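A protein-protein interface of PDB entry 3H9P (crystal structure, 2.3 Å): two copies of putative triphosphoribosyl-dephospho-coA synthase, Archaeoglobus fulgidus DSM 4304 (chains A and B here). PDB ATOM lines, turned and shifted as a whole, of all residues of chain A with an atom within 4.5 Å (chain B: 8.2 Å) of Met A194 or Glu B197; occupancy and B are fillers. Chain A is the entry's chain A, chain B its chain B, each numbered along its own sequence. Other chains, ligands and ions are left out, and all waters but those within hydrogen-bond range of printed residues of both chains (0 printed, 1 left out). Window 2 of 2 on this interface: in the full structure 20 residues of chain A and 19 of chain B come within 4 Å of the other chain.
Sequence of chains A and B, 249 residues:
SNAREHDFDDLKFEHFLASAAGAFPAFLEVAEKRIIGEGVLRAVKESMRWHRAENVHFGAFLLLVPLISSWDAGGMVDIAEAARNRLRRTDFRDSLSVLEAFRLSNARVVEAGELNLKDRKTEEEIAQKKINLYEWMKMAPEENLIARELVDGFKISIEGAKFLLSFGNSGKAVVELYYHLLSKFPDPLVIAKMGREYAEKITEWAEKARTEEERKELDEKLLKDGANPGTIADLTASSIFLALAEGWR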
ATOM      1  N   VAL A 190      29.511   3.622  14.543  1.00  0.00           N
ATOM      2  CA  VAL A 190      30.578   3.480  13.545  1.00  0.00           C
ATOM      3  C   VAL A 190      30.069   2.661  12.337  1.00  0.00           C
ATOM      4  O   VAL A 190      30.315   3.032  11.188  1.00  0.00           O
ATOM      5  CB  VAL A 190      31.832   2.863  14.176  1.00  0.00           C
ATOM      6  CG1 VAL A 190      32.855   2.483  13.124  1.00  0.00           C
ATOM      7  CG2 VAL A 190      32.416   3.793  15.218  1.00  0.00           C
ATOM      8  N   ILE A 191      29.357   1.553  12.598  1.00  0.00           N
ATOM      9  CA  ILE A 191      28.829   0.711  11.507  1.00  0.00           C
ATOM     10  C   ILE A 191      28.061   1.596  10.524  1.00  0.00           C
ATOM     11  O   ILE A 191      28.311   1.565   9.307  1.00  0.00           O
ATOM     12  CB  ILE A 191      27.889  -0.453  12.019  1.00  0.00           C
ATOM     13  CG1 ILE A 191      28.680  -1.528  12.784  1.00  0.00           C
ATOM     14  CG2 ILE A 191      27.164  -1.076  10.886  1.00  0.00           C
ATOM     15  CD1 ILE A 191      27.828  -2.559  13.496  1.00  0.00           C
ATOM     16  N   ALA A 192      27.164   2.422  11.065  1.00  0.00           N
ATOM     17  CA  ALA A 192      26.268   3.223  10.242  1.00  0.00           C
ATOM     18  C   ALA A 192      26.995   4.319   9.481  1.00  0.00           C
ATOM     19  O   ALA A 192      26.566   4.707   8.417  1.00  0.00           O
ATOM     20  CB  ALA A 192      25.144   3.817  11.109  1.00  0.00           C
ATOM     21  N   LYS A 193      28.081   4.844  10.039  1.00  0.00           N
ATOM     22  CA  LYS A 193      28.813   5.937   9.379  1.00  0.00           C
ATOM     23  C   LYS A 193      29.897   5.417   8.420  1.00  0.00           C
ATOM     24  O   LYS A 193      29.985   5.877   7.278  1.00  0.00           O
ATOM     25  CB  LYS A 193      29.445   6.888  10.412  1.00  0.00           C
ATOM     26  CG  LYS A 193      30.117   8.103   9.784  1.00  0.00           C
ATOM     27  CD  LYS A 193      30.519   9.139  10.804  1.00  0.00           C
ATOM     28  CE  LYS A 193      30.969  10.426  10.103  1.00  0.00           C
ATOM     29  NZ  LYS A 193      30.661  11.653  10.920  1.00  0.00           N
ATOM     30  N   MET A 194      30.708   4.471   8.915  1.00  0.00           N
ATOM     31  CA  MET A 194      31.895   3.960   8.223  1.00  0.00           C
ATOM     32  C   MET A 194      31.707   2.599   7.584  1.00  0.00           C
ATOM     33  O   MET A 194      32.527   2.185   6.778  1.00  0.00           O
ATOM     34  CB  MET A 194      33.073   3.828   9.190  1.00  0.00           C
ATOM     35  CG  MET A 194      33.353   5.011  10.045  1.00  0.00           C
ATOM     36  SD  MET A 194      33.476   6.647   9.043  1.00  0.00           S
ATOM     37  CE  MET A 194      34.995   6.283   7.832  1.00  0.00           C
ATOM     38  N   GLY A 195      30.659   1.882   7.965  1.00  0.00           N
ATOM     39  CA  GLY A 195      30.441   0.552   7.434  1.00  0.00           C
ATOM     40  C   GLY A 195      30.868  -0.551   8.383  1.00  0.00           C
ATOM     41  O   GLY A 195      31.713  -0.358   9.243  1.00  0.00           O
ATOM     42  N   TYR A 198      34.674  -1.437   8.738  1.00  0.00           N
ATOM     43  CA  TYR A 198      35.488  -0.476   9.473  1.00  0.00           C
ATOM     44  C   TYR A 198      35.215  -0.589  10.974  1.00  0.00           C
ATOM     45  O   TYR A 198      36.139  -0.571  11.787  1.00  0.00           O
ATOM     46  CB  TYR A 198      35.251   0.963   8.973  1.00  0.00           C
ATOM     47  CG  TYR A 198      36.173   1.981   9.600  1.00  0.00           C
ATOM     48  CD1 TYR A 198      37.192   2.595   8.857  1.00  0.00           C
ATOM     49  CD2 TYR A 198      36.030   2.333  10.933  1.00  0.00           C
ATOM     50  CE1 TYR A 198      38.050   3.518   9.455  1.00  0.00           C
ATOM     51  CE2 TYR A 198      36.876   3.255  11.537  1.00  0.00           C
ATOM     52  CZ  TYR A 198      37.874   3.835  10.808  1.00  0.00           C
ATOM     53  OH  TYR A 198      38.674   4.734  11.451  1.00  0.00           O
ATOM     54  N   ASP A 225      39.561  10.006  10.864  1.00  0.00           N
ATOM     55  CA  ASP A 225      38.543   9.306  10.093  1.00  0.00           C
ATOM     56  C   ASP A 225      37.113   9.794  10.305  1.00  0.00           C
ATOM     57  O   ASP A 225      36.253   9.520   9.465  1.00  0.00           O
ATOM     58  CB  ASP A 225      38.622   7.801  10.331  1.00  0.00           C
ATOM     59  CG  ASP A 225      39.797   7.179   9.622  1.00  0.00           C
ATOM     60  OD1 ASP A 225      40.471   7.901   8.866  1.00  0.00           O
ATOM     61  OD2 ASP A 225      40.062   5.982   9.814  1.00  0.00           O
ATOM     62  N   ALA A 227      35.368   8.822  12.926  1.00  0.00           N
ATOM     63  CA  ALA A 227      34.713   7.648  13.501  1.00  0.00           C
ATOM     64  C   ALA A 227      34.696   7.728  15.020  1.00  0.00           C
ATOM     65  O   ALA A 227      35.722   7.506  15.639  1.00  0.00           O
ATOM     66  CB  ALA A 227      35.451   6.388  13.062  1.00  0.00           C
ATOM     67  N   PRO B 186      20.905   7.295  -2.333  1.00  0.00           N
ATOM     68  CA  PRO B 186      21.912   6.474  -1.676  1.00  0.00           C
ATOM     69  C   PRO B 186      21.349   5.045  -1.429  1.00  0.00           C
ATOM     70  O   PRO B 186      20.193   4.898  -1.018  1.00  0.00           O
ATOM     71  CB  PRO B 186      22.137   7.204  -0.341  1.00  0.00           C
ATOM     72  CG  PRO B 186      21.414   8.494  -0.460  1.00  0.00           C
ATOM     73  CD  PRO B 186      20.306   8.251  -1.391  1.00  0.00           C
ATOM     74  N   VAL B 190      24.380  -0.526   0.267  1.00  0.00           N
ATOM     75  CA  VAL B 190      25.700   0.072   0.351  1.00  0.00           C
ATOM     76  C   VAL B 190      25.897   0.777   1.721  1.00  0.00           C
ATOM     77  O   VAL B 190      26.888   0.562   2.400  1.00  0.00           O
ATOM     78  CB  VAL B 190      26.002   0.979  -0.878  1.00  0.00           C
ATOM     79  CG1 VAL B 190      27.311   1.693  -0.697  1.00  0.00           C
ATOM     80  CG2 VAL B 190      26.046   0.141  -2.147  1.00  0.00           C
ATOM     81  N   ILE B 191      24.932   1.587   2.148  1.00  0.00           N
ATOM     82  CA  ILE B 191      25.030   2.198   3.485  1.00  0.00           C
ATOM     83  C   ILE B 191      25.441   1.142   4.516  1.00  0.00           C
ATOM     84  O   ILE B 191      26.485   1.279   5.138  1.00  0.00           O
ATOM     85  CB  ILE B 191      23.712   2.926   3.920  1.00  0.00           C
ATOM     86  CG1 ILE B 191      23.523   4.216   3.112  1.00  0.00           C
ATOM     87  CG2 ILE B 191      23.743   3.273   5.397  1.00  0.00           C
ATOM     88  CD1 ILE B 191      22.126   4.785   3.151  1.00  0.00           C
ATOM     89  N   ALA B 192      24.648   0.075   4.656  1.00  0.00           N
ATOM     90  CA  ALA B 192      24.842  -0.937   5.701  1.00  0.00           C
ATOM     91  C   ALA B 192      26.204  -1.637   5.676  1.00  0.00           C
ATOM     92  O   ALA B 192      26.688  -2.093   6.711  1.00  0.00           O
ATOM     93  CB  ALA B 192      23.728  -1.954   5.660  1.00  0.00           C
ATOM     94  N   LYS B 193      26.824  -1.705   4.505  1.00  0.00           N
ATOM     95  CA  LYS B 193      28.087  -2.406   4.351  1.00  0.00           C
ATOM     96  C   LYS B 193      29.272  -1.449   4.461  1.00  0.00           C
ATOM     97  O   LYS B 193      30.195  -1.689   5.246  1.00  0.00           O
ATOM     98  CB  LYS B 193      28.115  -3.141   3.006  1.00  0.00           C
ATOM     99  CG  LYS B 193      29.301  -4.060   2.812  1.00  0.00           C
ATOM    100  CD  LYS B 193      29.067  -5.020   1.675  1.00  0.00           C
ATOM    101  CE  LYS B 193      30.001  -6.222   1.805  1.00  0.00           C
ATOM    102  NZ  LYS B 193      30.052  -7.022   0.542  1.00  0.00           N
ATOM    103  N   MET B 194      29.223  -0.381   3.665  1.00  0.00           N
ATOM    104  CA  MET B 194      30.307   0.590   3.541  1.00  0.00           C
ATOM    105  C   MET B 194      30.035   1.874   4.306  1.00  0.00           C
ATOM    106  O   MET B 194      30.900   2.738   4.399  1.00  0.00           O
ATOM    107  CB  MET B 194      30.490   0.968   2.077  1.00  0.00           C
ATOM    108  CG  MET B 194      30.266  -0.153   1.111  1.00  0.00           C
ATOM    109  SD  MET B 194      31.581  -1.522   1.450  1.00  0.00           S
ATOM    110  CE  MET B 194      33.187  -0.608   0.796  1.00  0.00           C
ATOM    111  N   GLY B 195      28.819   2.019   4.815  1.00  0.00           N
ATOM    112  CA  GLY B 195      28.463   3.196   5.592  1.00  0.00           C
ATOM    113  C   GLY B 195      27.982   4.387   4.788  1.00  0.00           C
ATOM    114  O   GLY B 195      28.269   4.527   3.599  1.00  0.00           O
ATOM    115  N   ARG B 196      27.272   5.258   5.483  1.00  0.00           N
ATOM    116  CA  ARG B 196      26.607   6.433   4.929  1.00  0.00           C
ATOM    117  C   ARG B 196      27.471   7.267   3.972  1.00  0.00           C
ATOM    118  O   ARG B 196      26.971   7.833   3.003  1.00  0.00           O
ATOM    119  CB  ARG B 196      26.129   7.299   6.096  1.00  0.00           C
ATOM    120  CG  ARG B 196      24.898   8.103   5.797  1.00  0.00           C
ATOM    121  CD  ARG B 196      24.234   8.586   7.063  1.00  0.00           C
ATOM    122  NE  ARG B 196      23.819   7.497   7.934  1.00  0.00           N
ATOM    123  CZ  ARG B 196      23.079   7.652   9.033  1.00  0.00           C
ATOM    124  NH1 ARG B 196      22.658   8.863   9.390  1.00  0.00           N
ATOM    125  NH2 ARG B 196      22.756   6.597   9.773  1.00  0.00           N
ATOM    126  N   GLU B 197      28.766   7.324   4.254  1.00  0.00           N
ATOM    127  CA  GLU B 197      29.709   8.178   3.535  1.00  0.00           C
ATOM    128  C   GLU B 197      29.980   7.670   2.114  1.00  0.00           C
ATOM    129  O   GLU B 197      29.823   8.404   1.137  1.00  0.00           O
ATOM    130  CB  GLU B 197      31.010   8.240   4.327  1.00  0.00           C
ATOM    131  CG  GLU B 197      31.945   9.369   3.963  1.00  0.00           C
ATOM    132  CD  GLU B 197      33.235   9.275   4.741  1.00  0.00           C
ATOM    133  OE1 GLU B 197      33.193   8.846   5.925  1.00  0.00           O
ATOM    134  OE2 GLU B 197      34.291   9.623   4.167  1.00  0.00           O
ATOM    135  N   TYR B 198      30.401   6.411   2.027  1.00  0.00           N
ATOM    136  CA  TYR B 198      30.668   5.734   0.770  1.00  0.00           C
ATOM    137  C   TYR B 198      29.430   5.754  -0.147  1.00  0.00           C
ATOM    138  O   TYR B 198      29.522   6.119  -1.309  1.00  0.00           O
ATOM    139  CB  TYR B 198      31.109   4.301   1.075  1.00  0.00           C
ATOM    140  CG  TYR B 198      31.655   3.561  -0.112  1.00  0.00           C
ATOM    141  CD1 TYR B 198      33.032   3.473  -0.337  1.00  0.00           C
ATOM    142  CD2 TYR B 198      30.799   2.946  -1.014  1.00  0.00           C
ATOM    143  CE1 TYR B 198      33.531   2.787  -1.443  1.00  0.00           C
ATOM    144  CE2 TYR B 198      31.284   2.268  -2.125  1.00  0.00           C
ATOM    145  CZ  TYR B 198      32.632   2.185  -2.331  1.00  0.00           C
ATOM    146  OH  TYR B 198      33.069   1.500  -3.427  1.00  0.00           O
ATOM    147  N   ALA B 199      28.277   5.378   0.398  1.00  0.00           N
ATOM    148  CA  ALA B 199      27.003   5.392  -0.315  1.00  0.00           C
ATOM    149  C   ALA B 199      26.634   6.776  -0.856  1.00  0.00           C
ATOM    150  O   ALA B 199      26.204   6.913  -1.992  1.00  0.00           O
ATOM    151  CB  ALA B 199      25.902   4.868   0.577  1.00  0.00           C
ATOM    152  N   GLU B 200      26.801   7.803  -0.038  1.00  0.00           N
ATOM    153  CA  GLU B 200      26.522   9.170  -0.462  1.00  0.00           C
ATOM    154  C   GLU B 200      27.439   9.503  -1.626  1.00  0.00           C
ATOM    155  O   GLU B 200      27.028  10.187  -2.567  1.00  0.00           O
ATOM    156  CB  GLU B 200      26.760  10.129   0.689  1.00  0.00           C
ATOM    157  CG  GLU B 200      25.964  11.406   0.634  1.00  0.00           C
ATOM    158  CD  GLU B 200      26.116  12.220   1.913  1.00  0.00           C
ATOM    159  OE1 GLU B 200      26.195  11.614   3.009  1.00  0.00           O
ATOM    160  OE2 GLU B 200      26.161  13.472   1.826  1.00  0.00           O
ATOM    161  N   LYS B 201      28.661   8.964  -1.579  1.00  0.00           N
ATOM    162  CA  LYS B 201      29.657   9.178  -2.635  1.00  0.00           C
ATOM    163  C   LYS B 201      29.291   8.508  -3.966  1.00  0.00           C
ATOM    164  O   LYS B 201      29.562   9.069  -5.032  1.00  0.00           O
ATOM    165  CB  LYS B 201      31.043   8.722  -2.173  1.00  0.00           C
ATOM    166  CG  LYS B 201      31.609   9.553  -1.010  1.00  0.00           C
ATOM    167  CD  LYS B 201      32.890   8.947  -0.449  1.00  0.00           C
ATOM    168  CE  LYS B 201      34.093   9.289  -1.312  1.00  0.00           C
ATOM    169  NZ  LYS B 201      34.420  10.735  -1.218  1.00  0.00           N
ATOM    170  N   ILE B 202      28.705   7.311  -3.898  1.00  0.00           N
ATOM    171  CA  ILE B 202      28.180   6.632  -5.084  1.00  0.00           C
ATOM    172  C   ILE B 202      27.287   7.582  -5.875  1.00  0.00           C
ATOM    173  O   ILE B 202      27.505   7.781  -7.058  1.00  0.00           O
ATOM    174  CB  ILE B 202      27.345   5.362  -4.745  1.00  0.00           C
ATOM    175  CG1 ILE B 202      28.159   4.356  -3.952  1.00  0.00           C
ATOM    176  CG2 ILE B 202      26.827   4.713  -6.005  1.00  0.00           C
ATOM    177  CD1 ILE B 202      29.312   3.789  -4.729  1.00  0.00           C
ATOM    178  N   THR B 203      26.296   8.176  -5.217  1.00  0.00           N
ATOM    179  CA  THR B 203      25.343   9.028  -5.931  1.00  0.00           C
ATOM    180  C   THR B 203      26.122  10.088  -6.674  1.00  0.00           C
ATOM    181  O   THR B 203      25.977  10.261  -7.883  1.00  0.00           O
ATOM    182  CB  THR B 203      24.288   9.679  -5.003  1.00  0.00           C
ATOM    183  OG1 THR B 203      24.897  10.689  -4.190  1.00  0.00           O
ATOM    184  CG2 THR B 203      23.653   8.636  -4.114  1.00  0.00           C
ATOM    185  N   GLU B 204      26.992  10.769  -5.946  1.00  0.00           N
ATOM    186  CA  GLU B 204      27.776  11.826  -6.538  1.00  0.00           C
ATOM    187  C   GLU B 204      28.668  11.276  -7.632  1.00  0.00           C
ATOM    188  O   GLU B 204      28.814  11.907  -8.684  1.00  0.00           O
ATOM    189  CB  GLU B 204      28.542  12.608  -5.474  1.00  0.00           C
ATOM    190  CG  GLU B 204      27.861  13.940  -5.144  1.00  0.00           C
ATOM    191  CD  GLU B 204      28.239  14.509  -3.785  1.00  0.00           C
ATOM    192  OE1 GLU B 204      28.641  13.729  -2.892  1.00  0.00           O
ATOM    193  OE2 GLU B 204      28.107  15.741  -3.601  1.00  0.00           O
ATOM    194  N   TRP B 205      29.232  10.089  -7.420  1.00  0.00           N
ATOM    195  CA  TRP B 205      30.017   9.474  -8.481  1.00  0.00           C
ATOM    196  C   TRP B 205      29.120   9.300  -9.707  1.00  0.00           C
ATOM    197  O   TRP B 205      29.381   9.917 -10.743  1.00  0.00           O
ATOM    198  CB  TRP B 205      30.646   8.138  -8.059  1.00  0.00           C
ATOM    199  CG  TRP B 205      31.967   8.224  -7.329  1.00  0.00           C
ATOM    200  CD1 TRP B 205      32.982   9.131  -7.543  1.00  0.00           C
ATOM    201  CD2 TRP B 205      32.432   7.346  -6.294  1.00  0.00           C
ATOM    202  NE1 TRP B 205      34.028   8.879  -6.689  1.00  0.00           N
ATOM    203  CE2 TRP B 205      33.722   7.791  -5.914  1.00  0.00           C
ATOM    204  CE3 TRP B 205      31.879   6.233  -5.639  1.00  0.00           C
ATOM    205  CZ2 TRP B 205      34.467   7.165  -4.908  1.00  0.00           C
ATOM    206  CZ3 TRP B 205      32.624   5.604  -4.639  1.00  0.00           C
ATOM    207  CH2 TRP B 205      33.903   6.079  -4.283  1.00  0.00           C
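The backbone carbonyl oxygen (O) of Val B190 is in hydrogen-bond range of the backbone NH (N) of Gly B195 (3.4 Å). The backbone carbonyl oxygen (O) of Val A190 sits at hydrogen-bond distance from the backbone NH (N) of Gly A195, at 3.4 Å.
Lys A193 touches Gly B195, and with the chains exchanged Gly A195 touches Lys B193. Met B194 touches its own counterpart, Met A194. Met A194 touches Gly B195, and with the chains exchanged Gly A195 touches Met B194. Gly B195 touches its own counterpart, Gly A195. 7 positions are printed for both chains.
The backbone carbonyl oxygen (O) of Met A194 lies close to the backbone carbonyl oxygen (O) of Met B194 (2.9 Å). The backbone carbonyl oxygen of Lys A193 is in hydrogen-bond range of the backbone NH of Arg B196 (3.3 Å). The backbone carbonyl oxygen (O) of Ala A192 is in hydrogen-bond range of the backbone NH (N) of Arg B196.
Among the printed residues, merely in contact across the chains: Ala A192 with Gly B195, Lys A193 with Gly B195, Lys A193 with Glu B197, Met A194 with Gly B195, Met A194 with Glu B197, Gly A195 with Lys B193, Gly A195 with Met B194 and Gly A195 with Gly B195.
Of the printed residues of chain B, Ala A192 touches Gly B195 and Arg B196. Of the printed residues of chain B, Lys A193 touches Gly B195 (3.5 Å), Arg B196 (3.3 Å) and Glu B197 (3.6 Å). Of chain B, only Met B194, Gly B195 and Glu B197 come within 4 Å of Met A194. Of chain B, only Lys B193 (3.1 Å), Met B194 (3.4 Å) and Gly B195 (3.4 Å) come within 4 Å of Gly A195. Printed residues of chain A within 4 Å of Met B194: Met A194 and Gly A195. The nearest residue of chain B that does not touch Met A194 is Lys B193 (4.8 Å). The nearest printed residue of chain A that does not touch Met B194 is Lys A193 (4.4 Å).
Printed residues of chain B that touch a printed residue of chain A: Lys B193, Met B194, Gly B195, Arg B196 and Glu B197. Along chain B the printed residues that touch a printed residue of chain A span positions 193 to 197. Of the 9 printed residues of chain A, 4 touch a printed residue of chain B. Hydrophobic or aromatic side chains of chain A that line the printed part of chain B: Ala A192 and Met A194. Along chain A the printed residues that touch a printed residue of chain B span positions 192 to 195. Among the printed residues, 11 pairs touch across the chains. Among the printed residues, no Asp or Glu carboxylate lies within 4 Å of a Lys or Arg side-chain nitrogen of the other chain.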
